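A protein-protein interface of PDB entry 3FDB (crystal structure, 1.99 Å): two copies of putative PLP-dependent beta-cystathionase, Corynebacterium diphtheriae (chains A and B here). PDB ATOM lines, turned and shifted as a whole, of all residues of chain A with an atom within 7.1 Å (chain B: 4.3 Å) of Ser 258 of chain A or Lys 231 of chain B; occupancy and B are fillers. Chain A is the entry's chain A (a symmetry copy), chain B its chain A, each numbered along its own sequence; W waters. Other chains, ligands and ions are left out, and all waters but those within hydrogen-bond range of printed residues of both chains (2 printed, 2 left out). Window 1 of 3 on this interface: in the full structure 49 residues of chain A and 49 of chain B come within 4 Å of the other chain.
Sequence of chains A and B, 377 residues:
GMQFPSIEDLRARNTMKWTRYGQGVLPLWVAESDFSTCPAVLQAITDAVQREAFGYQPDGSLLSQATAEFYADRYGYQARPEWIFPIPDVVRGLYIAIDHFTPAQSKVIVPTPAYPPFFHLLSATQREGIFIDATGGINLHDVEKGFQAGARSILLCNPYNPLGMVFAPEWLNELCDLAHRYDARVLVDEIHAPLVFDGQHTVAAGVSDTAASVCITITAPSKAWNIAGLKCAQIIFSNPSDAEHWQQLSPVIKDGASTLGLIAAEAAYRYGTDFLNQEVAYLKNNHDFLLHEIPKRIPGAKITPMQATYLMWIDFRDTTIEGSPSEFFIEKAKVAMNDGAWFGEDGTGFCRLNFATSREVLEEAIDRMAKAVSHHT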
ATOM      1  N   PHE A  54     -23.527 -35.875  13.017  1.00  0.00           N
ATOM      2  CA  PHE A  54     -24.640 -35.489  13.884  1.00  0.00           C
ATOM      3  C   PHE A  54     -24.346 -35.612  15.368  1.00  0.00           C
ATOM      4  O   PHE A  54     -25.236 -35.336  16.220  1.00  0.00           O
ATOM      5  CB  PHE A  54     -25.881 -36.358  13.567  1.00  0.00           C
ATOM      6  CG  PHE A  54     -26.307 -36.347  12.116  1.00  0.00           C
ATOM      7  CD1 PHE A  54     -26.206 -35.188  11.335  1.00  0.00           C
ATOM      8  CD2 PHE A  54     -26.855 -37.488  11.544  1.00  0.00           C
ATOM      9  CE1 PHE A  54     -26.626 -35.192  10.012  1.00  0.00           C
ATOM     10  CE2 PHE A  54     -27.269 -37.492  10.233  1.00  0.00           C
ATOM     11  CZ  PHE A  54     -27.157 -36.343   9.467  1.00  0.00           C
ATOM     12  N   GLY A  55     -23.127 -36.032  15.697  1.00  0.00           N
ATOM     13  CA  GLY A  55     -22.738 -36.202  17.101  1.00  0.00           C
ATOM     14  C   GLY A  55     -22.143 -34.910  17.620  1.00  0.00           C
ATOM     15  O   GLY A  55     -22.441 -33.835  17.109  1.00  0.00           O
ATOM     16  N   TYR A  56     -21.264 -35.019  18.606  1.00  0.00           N
ATOM     17  CA  TYR A  56     -20.646 -33.848  19.224  1.00  0.00           C
ATOM     18  C   TYR A  56     -19.548 -33.265  18.354  1.00  0.00           C
ATOM     19  O   TYR A  56     -18.986 -33.931  17.485  1.00  0.00           O
ATOM     20  CB  TYR A  56     -20.088 -34.198  20.601  1.00  0.00           C
ATOM     21  CG  TYR A  56     -21.173 -34.626  21.542  1.00  0.00           C
ATOM     22  CD1 TYR A  56     -22.082 -33.702  22.041  1.00  0.00           C
ATOM     23  CD2 TYR A  56     -21.333 -35.968  21.885  1.00  0.00           C
ATOM     24  CE1 TYR A  56     -23.100 -34.099  22.891  1.00  0.00           C
ATOM     25  CE2 TYR A  56     -22.351 -36.371  22.732  1.00  0.00           C
ATOM     26  CZ  TYR A  56     -23.226 -35.433  23.227  1.00  0.00           C
ATOM     27  OH  TYR A  56     -24.256 -35.839  24.059  1.00  0.00           O
ATOM     28  N   GLN A  57     -19.219 -32.012  18.602  1.00  0.00           N
ATOM     29  CA  GLN A  57     -18.261 -31.334  17.755  1.00  0.00           C
ATOM     30  C   GLN A  57     -16.879 -31.927  17.856  1.00  0.00           C
ATOM     31  O   GLN A  57     -16.448 -32.326  18.926  1.00  0.00           O
ATOM     32  CB  GLN A  57     -18.221 -29.843  18.065  1.00  0.00           C
ATOM     33  CG  GLN A  57     -17.601 -29.452  19.391  1.00  0.00           C
ATOM     34  CD  GLN A  57     -18.019 -28.022  19.767  1.00  0.00           C
ATOM     35  OE1 GLN A  57     -17.208 -27.098  19.717  1.00  0.00           O
ATOM     36  NE2 GLN A  57     -19.319 -27.827  20.058  1.00  0.00           N
ATOM     37  N   ILE A  87     -19.940 -19.941  19.876  1.00  0.00           N
ATOM     38  CA  ILE A  87     -21.097 -19.732  20.720  1.00  0.00           C
ATOM     39  C   ILE A  87     -22.292 -20.037  19.851  1.00  0.00           C
ATOM     40  O   ILE A  87     -22.206 -20.048  18.616  1.00  0.00           O
ATOM     41  CB  ILE A  87     -21.168 -18.251  21.262  1.00  0.00           C
ATOM     42  CG1 ILE A  87     -20.681 -17.247  20.197  1.00  0.00           C
ATOM     43  CG2 ILE A  87     -20.292 -18.108  22.506  1.00  0.00           C
ATOM     44  CD1 ILE A  87     -21.003 -15.758  20.470  1.00  0.00           C
ATOM     45  N   PRO A  88     -23.440 -20.295  20.470  1.00  0.00           N
ATOM     46  CA  PRO A  88     -24.610 -20.622  19.642  1.00  0.00           C
ATOM     47  C   PRO A  88     -25.148 -19.519  18.746  1.00  0.00           C
ATOM     48  O   PRO A  88     -25.673 -19.790  17.629  1.00  0.00           O
ATOM     49  CB  PRO A  88     -25.686 -20.999  20.663  1.00  0.00           C
ATOM     50  CG  PRO A  88     -25.152 -20.765  21.953  1.00  0.00           C
ATOM     51  CD  PRO A  88     -23.704 -20.396  21.905  1.00  0.00           C
ATOM     52  N   GLY A 229     -30.511 -20.304  11.582  1.00  0.00           N
ATOM     53  CA  GLY A 229     -31.059 -21.466  12.265  1.00  0.00           C
ATOM     54  C   GLY A 229     -30.054 -22.563  12.562  1.00  0.00           C
ATOM     55  O   GLY A 229     -30.414 -23.559  13.178  1.00  0.00           O
ATOM     56  N   LEU A 230     -28.810 -22.412  12.099  1.00  0.00           N
ATOM     57  CA  LEU A 230     -27.791 -23.416  12.318  1.00  0.00           C
ATOM     58  C   LEU A 230     -26.958 -23.172  13.569  1.00  0.00           C
ATOM     59  O   LEU A 230     -26.130 -24.009  13.939  1.00  0.00           O
ATOM     60  CB  LEU A 230     -26.877 -23.581  11.085  1.00  0.00           C
ATOM     61  CG  LEU A 230     -27.425 -24.418   9.904  1.00  0.00           C
ATOM     62  CD1 LEU A 230     -28.603 -23.795   9.274  1.00  0.00           C
ATOM     63  CD2 LEU A 230     -26.407 -24.585   8.832  1.00  0.00           C
ATOM     64  N   LYS A 231     -27.188 -22.056  14.245  1.00  0.00           N
ATOM     65  CA  LYS A 231     -26.555 -21.818  15.543  1.00  0.00           C
ATOM     66  C   LYS A 231     -25.005 -21.910  15.600  1.00  0.00           C
ATOM     67  O   LYS A 231     -24.416 -22.851  16.170  1.00  0.00           O
ATOM     68  CB  LYS A 231     -27.146 -22.742  16.636  1.00  0.00           C
ATOM     69  CG  LYS A 231     -28.668 -22.855  16.685  1.00  0.00           C
ATOM     70  CD  LYS A 231     -29.438 -21.510  16.696  1.00  0.00           C
ATOM     71  CE  LYS A 231     -29.133 -20.676  17.911  1.00  0.00           C
ATOM     72  NZ  LYS A 231     -30.032 -19.521  18.000  1.00  0.00           N
ATOM     73  N   CYS A 232     -24.349 -20.902  15.040  1.00  0.00           N
ATOM     74  CA  CYS A 232     -22.913 -20.779  15.180  1.00  0.00           C
ATOM     75  C   CYS A 232     -22.509 -19.340  15.018  1.00  0.00           C
ATOM     76  O   CYS A 232     -22.673 -18.767  13.967  1.00  0.00           O
ATOM     77  CB  CYS A 232     -22.159 -21.640  14.169  1.00  0.00           C
ATOM     78  SG  CYS A 232     -20.368 -21.514  14.441  1.00  0.00           S
ATOM     79  N   ASP A 255     -21.610 -23.535  26.002  1.00  0.00           N
ATOM     80  CA  ASP A 255     -21.935 -24.480  24.963  1.00  0.00           C
ATOM     81  C   ASP A 255     -23.261 -24.132  24.289  1.00  0.00           C
ATOM     82  O   ASP A 255     -23.996 -23.261  24.757  1.00  0.00           O
ATOM     83  CB  ASP A 255     -21.906 -25.908  25.515  1.00  0.00           C
ATOM     84  CG  ASP A 255     -20.492 -26.366  25.929  1.00  0.00           C
ATOM     85  OD1 ASP A 255     -19.478 -25.629  25.757  1.00  0.00           O
ATOM     86  OD2 ASP A 255     -20.404 -27.469  26.485  1.00  0.00           O
ATOM     87  N   GLY A 256     -23.535 -24.788  23.166  1.00  0.00           N
ATOM     88  CA  GLY A 256     -24.750 -24.557  22.392  1.00  0.00           C
ATOM     89  C   GLY A 256     -24.628 -24.597  20.905  1.00  0.00           C
ATOM     90  O   GLY A 256     -25.609 -24.869  20.229  1.00  0.00           O
ATOM     91  N   ALA A 257     -23.441 -24.344  20.372  1.00  0.00           N
ATOM     92  CA  ALA A 257     -23.286 -24.283  18.925  1.00  0.00           C
ATOM     93  C   ALA A 257     -23.591 -25.644  18.344  1.00  0.00           C
ATOM     94  O   ALA A 257     -23.299 -26.656  18.963  1.00  0.00           O
ATOM     95  CB  ALA A 257     -21.853 -23.835  18.544  1.00  0.00           C
ATOM     96  N   SER A 258     -24.203 -25.673  17.168  1.00  0.00           N
ATOM     97  CA  SER A 258     -24.512 -26.929  16.528  1.00  0.00           C
ATOM     98  C   SER A 258     -23.361 -27.407  15.639  1.00  0.00           C
ATOM     99  O   SER A 258     -22.577 -26.620  15.090  1.00  0.00           O
ATOM    100  CB  SER A 258     -25.850 -26.861  15.758  1.00  0.00           C
ATOM    101  OG  SER A 258     -25.694 -26.524  14.393  1.00  0.00           O
ATOM    102  N   THR A 259     -23.282 -28.723  15.499  1.00  0.00           N
ATOM    103  CA  THR A 259     -22.220 -29.362  14.743  1.00  0.00           C
ATOM    104  C   THR A 259     -22.238 -28.943  13.263  1.00  0.00           C
ATOM    105  O   THR A 259     -21.184 -28.567  12.671  1.00  0.00           O
ATOM    106  CB  THR A 259     -22.314 -30.911  14.957  1.00  0.00           C
ATOM    107  OG1 THR A 259     -22.031 -31.166  16.340  1.00  0.00           O
ATOM    108  CG2 THR A 259     -21.283 -31.672  14.155  1.00  0.00           C
ATOM    109  N   LEU A 260     -23.432 -28.988  12.675  1.00  0.00           N
ATOM    110  CA  LEU A 260     -23.661 -28.523  11.320  1.00  0.00           C
ATOM    111  C   LEU A 260     -23.411 -27.037  11.190  1.00  0.00           C
ATOM    112  O   LEU A 260     -22.883 -26.579  10.177  1.00  0.00           O
ATOM    113  CB  LEU A 260     -25.082 -28.864  10.855  1.00  0.00           C
ATOM    114  CG  LEU A 260     -25.338 -30.354  10.645  1.00  0.00           C
ATOM    115  CD1 LEU A 260     -26.816 -30.602  10.209  1.00  0.00           C
ATOM    116  CD2 LEU A 260     -24.381 -30.917   9.620  1.00  0.00           C
ATOM    117  N   GLY A 261     -23.757 -26.276  12.222  1.00  0.00           N
ATOM    118  CA  GLY A 261     -23.500 -24.835  12.190  1.00  0.00           C
ATOM    119  C   GLY A 261     -22.014 -24.484  12.168  1.00  0.00           C
ATOM    120  O   GLY A 261     -21.609 -23.542  11.498  1.00  0.00           O
ATOM    121  N   LEU A 262     -21.198 -25.221  12.909  1.00  0.00           N
ATOM    122  CA  LEU A 262     -19.746 -25.018  12.894  1.00  0.00           C
ATOM    123  C   LEU A 262     -19.212 -25.246  11.486  1.00  0.00           C
ATOM    124  O   LEU A 262     -18.393 -24.473  10.980  1.00  0.00           O
ATOM    125  CB  LEU A 262     -19.040 -25.971  13.875  1.00  0.00           C
ATOM    126  CG  LEU A 262     -19.328 -25.715  15.373  1.00  0.00           C
ATOM    127  CD1 LEU A 262     -19.067 -26.930  16.268  1.00  0.00           C
ATOM    128  CD2 LEU A 262     -18.531 -24.541  15.839  1.00  0.00           C
ATOM    129  N   ILE A 263     -19.712 -26.292  10.843  1.00  0.00           N
ATOM    130  CA  ILE A 263     -19.304 -26.642   9.486  1.00  0.00           C
ATOM    131  C   ILE A 263     -19.747 -25.565   8.461  1.00  0.00           C
ATOM    132  O   ILE A 263     -18.947 -25.140   7.632  1.00  0.00           O
ATOM    133  CB  ILE A 263     -19.882 -28.021   9.065  1.00  0.00           C
ATOM    134  CG1 ILE A 263     -19.167 -29.161   9.817  1.00  0.00           C
ATOM    135  CG2 ILE A 263     -19.729 -28.203   7.562  1.00  0.00           C
ATOM    136  CD1 ILE A 263     -19.951 -30.496   9.834  1.00  0.00           C
ATOM    137  N   ALA A 264     -21.008 -25.129   8.535  1.00  0.00           N
ATOM    138  CA  ALA A 264     -21.544 -24.080   7.640  1.00  0.00           C
ATOM    139  C   ALA A 264     -20.770 -22.749   7.796  1.00  0.00           C
ATOM    140  O   ALA A 264     -20.390 -22.112   6.797  1.00  0.00           O
ATOM    141  CB  ALA A 264     -23.052 -23.871   7.922  1.00  0.00           C
ATOM    142  N   PRO B  88     -32.314 -26.030  23.620  1.00  0.00           N
ATOM    143  CA  PRO B  88     -31.187 -26.531  22.820  1.00  0.00           C
ATOM    144  C   PRO B  88     -30.664 -27.916  23.162  1.00  0.00           C
ATOM    145  O   PRO B  88     -30.192 -28.670  22.265  1.00  0.00           O
ATOM    146  CB  PRO B  88     -30.078 -25.507  23.071  1.00  0.00           C
ATOM    147  CG  PRO B  88     -30.553 -24.592  24.041  1.00  0.00           C
ATOM    148  CD  PRO B  88     -31.993 -24.816  24.371  1.00  0.00           C
ATOM    149  N   ASP B  89     -30.696 -28.237  24.451  1.00  0.00           N
ATOM    150  CA  ASP B  89     -30.213 -29.524  24.930  1.00  0.00           C
ATOM    151  C   ASP B  89     -30.661 -29.770  26.375  1.00  0.00           C
ATOM    152  O   ASP B  89     -31.101 -28.851  27.046  1.00  0.00           O
ATOM    153  CB  ASP B  89     -28.690 -29.681  24.786  1.00  0.00           C
ATOM    154  CG  ASP B  89     -27.917 -28.584  25.468  1.00  0.00           C
ATOM    155  OD1 ASP B  89     -27.955 -28.542  26.709  1.00  0.00           O
ATOM    156  OD2 ASP B  89     -27.239 -27.800  24.760  1.00  0.00           O
ATOM    157  N   ILE B 227     -28.466 -37.692  17.456  1.00  0.00           N
ATOM    158  CA  ILE B 227     -28.478 -36.376  16.834  1.00  0.00           C
ATOM    159  C   ILE B 227     -28.098 -35.261  17.822  1.00  0.00           C
ATOM    160  O   ILE B 227     -28.551 -34.137  17.697  1.00  0.00           O
ATOM    161  CB  ILE B 227     -29.850 -36.124  16.130  1.00  0.00           C
ATOM    162  CG1 ILE B 227     -31.034 -36.448  17.063  1.00  0.00           C
ATOM    163  CG2 ILE B 227     -29.935 -36.941  14.809  1.00  0.00           C
ATOM    164  CD1 ILE B 227     -32.414 -36.077  16.481  1.00  0.00           C
ATOM    165  N   ALA B 228     -27.214 -35.559  18.771  1.00  0.00           N
ATOM    166  CA  ALA B 228     -26.809 -34.594  19.810  1.00  0.00           C
ATOM    167  C   ALA B 228     -26.303 -33.295  19.215  1.00  0.00           C
ATOM    168  O   ALA B 228     -26.555 -32.214  19.755  1.00  0.00           O
ATOM    169  CB  ALA B 228     -25.727 -35.192  20.753  1.00  0.00           C
ATOM    170  N   GLY B 229     -25.622 -33.354  18.091  1.00  0.00           N
ATOM    171  CA  GLY B 229     -25.071 -32.130  17.532  1.00  0.00           C
ATOM    172  C   GLY B 229     -26.085 -31.222  16.862  1.00  0.00           C
ATOM    173  O   GLY B 229     -25.721 -30.145  16.406  1.00  0.00           O
ATOM    174  N   LEU B 230     -27.344 -31.658  16.764  1.00  0.00           N
ATOM    175  CA  LEU B 230     -28.374 -30.868  16.124  1.00  0.00           C
ATOM    176  C   LEU B 230     -29.149 -29.984  17.091  1.00  0.00           C
ATOM    177  O   LEU B 230     -29.978 -29.174  16.667  1.00  0.00           O
ATOM    178  CB  LEU B 230     -29.342 -31.747  15.304  1.00  0.00           C
ATOM    179  CG  LEU B 230     -28.862 -32.221  13.911  1.00  0.00           C
ATOM    180  CD1 LEU B 230     -27.698 -33.121  13.994  1.00  0.00           C
ATOM    181  CD2 LEU B 230     -29.927 -32.966  13.188  1.00  0.00           C
ATOM    182  N   LYS B 231     -28.868 -30.101  18.381  1.00  0.00           N
ATOM    183  CA  LYS B 231     -29.441 -29.178  19.363  1.00  0.00           C
ATOM    184  C   LYS B 231     -30.988 -29.046  19.387  1.00  0.00           C
ATOM    185  O   LYS B 231     -31.572 -28.018  18.986  1.00  0.00           O
ATOM    186  CB  LYS B 231     -28.824 -27.764  19.235  1.00  0.00           C
ATOM    187  CG  LYS B 231     -27.304 -27.690  19.109  1.00  0.00           C
ATOM    188  CD  LYS B 231     -26.506 -28.490  20.169  1.00  0.00           C
ATOM    189  CE  LYS B 231     -26.743 -27.993  21.571  1.00  0.00           C
ATOM    190  NZ  LYS B 231     -25.817 -28.621  22.518  1.00  0.00           N
ATOM    191  N   CYS B 232     -31.645 -30.077  19.899  1.00  0.00           N
ATOM    192  CA  CYS B 232     -33.072 -30.007  20.140  1.00  0.00           C
ATOM    193  C   CYS B 232     -33.452 -30.976  21.224  1.00  0.00           C
ATOM    194  O   CYS B 232     -33.320 -32.167  21.062  1.00  0.00           O
ATOM    195  CB  CYS B 232     -33.885 -30.300  18.882  1.00  0.00           C
ATOM    196  SG  CYS B 232     -35.660 -30.116  19.218  1.00  0.00           S
ATOM    197  N   ALA B 257     -32.403 -23.723  20.292  1.00  0.00           N
ATOM    198  CA  ALA B 257     -32.617 -24.925  19.497  1.00  0.00           C
ATOM    199  C   ALA B 257     -32.366 -24.599  18.042  1.00  0.00           C
ATOM    200  O   ALA B 257     -32.653 -23.496  17.602  1.00  0.00           O
ATOM    201  CB  ALA B 257     -34.055 -25.466  19.694  1.00  0.00           C
ATOM    202  N   SER B 258     -31.803 -25.545  17.303  1.00  0.00           N
ATOM    203  CA  SER B 258     -31.549 -25.329  15.899  1.00  0.00           C
ATOM    204  C   SER B 258     -32.746 -25.741  15.037  1.00  0.00           C
ATOM    205  O   SER B 258     -33.535 -26.631  15.384  1.00  0.00           O
ATOM    206  CB  SER B 258     -30.242 -26.018  15.445  1.00  0.00           C
ATOM    207  OG  SER B 258     -30.449 -27.317  14.921  1.00  0.00           O
HETATM  208  O   HOH W   1     -32.455 -20.809  18.539  1.00  0.00           O
HETATM  209  O   HOH W   2     -23.400 -27.478  21.694  1.00  0.00           O
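O of Phe 54 of chain A sits at hydrogen-bond distance from N of Gly 229 of chain B (2.8 Å). The backbone NH of Gly 229 of chain B lies close to the backbone carbonyl oxygen of Gly 55 of chain A (3.4 Å). The backbone carbonyl oxygen (O) of Gly 229 of chain B sits at hydrogen-bond distance from the backbone NH (N) of Thr 259 of chain A, 3.0 Å away. O of Phe 54 of chain A sits at hydrogen-bond distance from N of Ala 228 of chain B (3.2 Å).
Of the 20 printed residues of chain A, 9 touch a printed residue of chain B. Hydrophobic or aromatic side chains of chain B within 4 Å of the printed part of chain A: Ala 228 and Leu 230. Among the printed residues, no Asp or Glu carboxylate lies within 4 Å of a Lys or Arg side-chain nitrogen of the other chain.
Water W1 bridges NZ of Lys 231 of chain A and O of Ala 257 of chain B. Water W2 lies within hydrogen-bond range of the side-chain amino group (NZ) of Lys 231 of chain B (2.8 Å), the backbone carbonyl oxygen (O) of Ala 257 of chain A (2.9 Å) and the backbone NH (N) of Gly 256 of chain A (3.1 Å).
Among the printed residues, merely in contact across the chains: Phe 54 of chain A with Ile 227 of chain B (3.3 Å), Gly 229 of chain A with Ser 258 of chain B (3.3 Å), Ser 258 of chain A with Gly 229 of chain B (3.3 Å), Gly 256 of chain A with Lys 231 of chain B (3.5 Å), Tyr 56 of chain A with Ala 228 of chain B (3.5 Å), Phe 54 of chain A with Leu 230 of chain B (3.7 Å), Lys 231 of chain A with Ser 258 of chain B (3.7 Å), Ser 258 of chain A with Lys 231 of chain B (3.7 Å), Lys 231 of chain A with Ala 257 of chain B (3.9 Å) and Ala 257 of chain A with Lys 231 of chain B (3.9 Å).
Gly 229 of chain A touches Ser 258 of chain B, and with the chains exchanged Ser 258 of chain A touches Gly 229 of chain B. Lys 231 of chain A touches Ala 257 of chain B, and with the chains exchanged Ala 257 of chain A touches Lys 231 of chain B. Lys 231 of chain A touches Ser 258 of chain B, and with the chains exchanged Ser 258 of chain A touches Lys 231 of chain B.
The backbone carbonyl oxygen of Leu 230 of chain B is in hydrogen-bond range of the side-chain hydroxyl of Ser 258 of chain B (2.6 Å). O of Lys 231 of chain A sits at hydrogen-bond distance from N of Ser 258 of chain A (3.0 Å). The backbone carbonyl oxygen (O) of Lys 231 of chain B is in hydrogen-bond range of the backbone NH (N) of Ser 258 of chain B. The side-chain hydroxyl of Ser 258 of chain A is in hydrogen-bond range of the backbone carbonyl oxygen of Leu 230 of chain A, 2.6 Å away. The side-chain hydroxyl (OG) of Ser 258 of chain A sits at hydrogen-bond distance from the backbone NH (N) of Gly 261 of chain A (2.9 Å). The side-chain hydroxyl of Thr 259 of chain A lies within hydrogen-bond range of the backbone carbonyl oxygen of Gly 55 of chain A (2.8 Å).
Of the printed residues of chain B, Gly 55 of chain A touches Gly 229 (3.2 Å). Of the printed residues of chain B, Tyr 56 of chain A touches Ala 228. Printed residues of chain B within 4 Å of Gly 256 of chain A: Lys 231 (3.5 Å). Ser 258 of chain A touches just these residues of chain B: Gly 229 (3.3 Å) and Lys 231 (3.7 Å). Leu 262 of chain A touches none of the printed residues of chain B. Ala 264 of chain A touches none of the printed residues of chain B. Printed residues of chain A within 4 Å of Leu 230 of chain B: Phe 54. Of the printed residues of chain A, Lys 231 of chain B touches Gly 256 (3.5 Å), Ala 257 (3.9 Å) and Ser 258 (3.7 Å). Printed residues of chain A within 4 Å of Ser 258 of chain B: Gly 229 (3.3 Å) and Lys 231 (3.7 Å). The nearest printed residue of chain B that does not touch Ser 258 of chain A is Ser 258 of chain B (4.5 Å). The nearest printed residue of chain A that does not touch Ile 227 of chain B is Gly 55 of chain A (5.5 Å).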
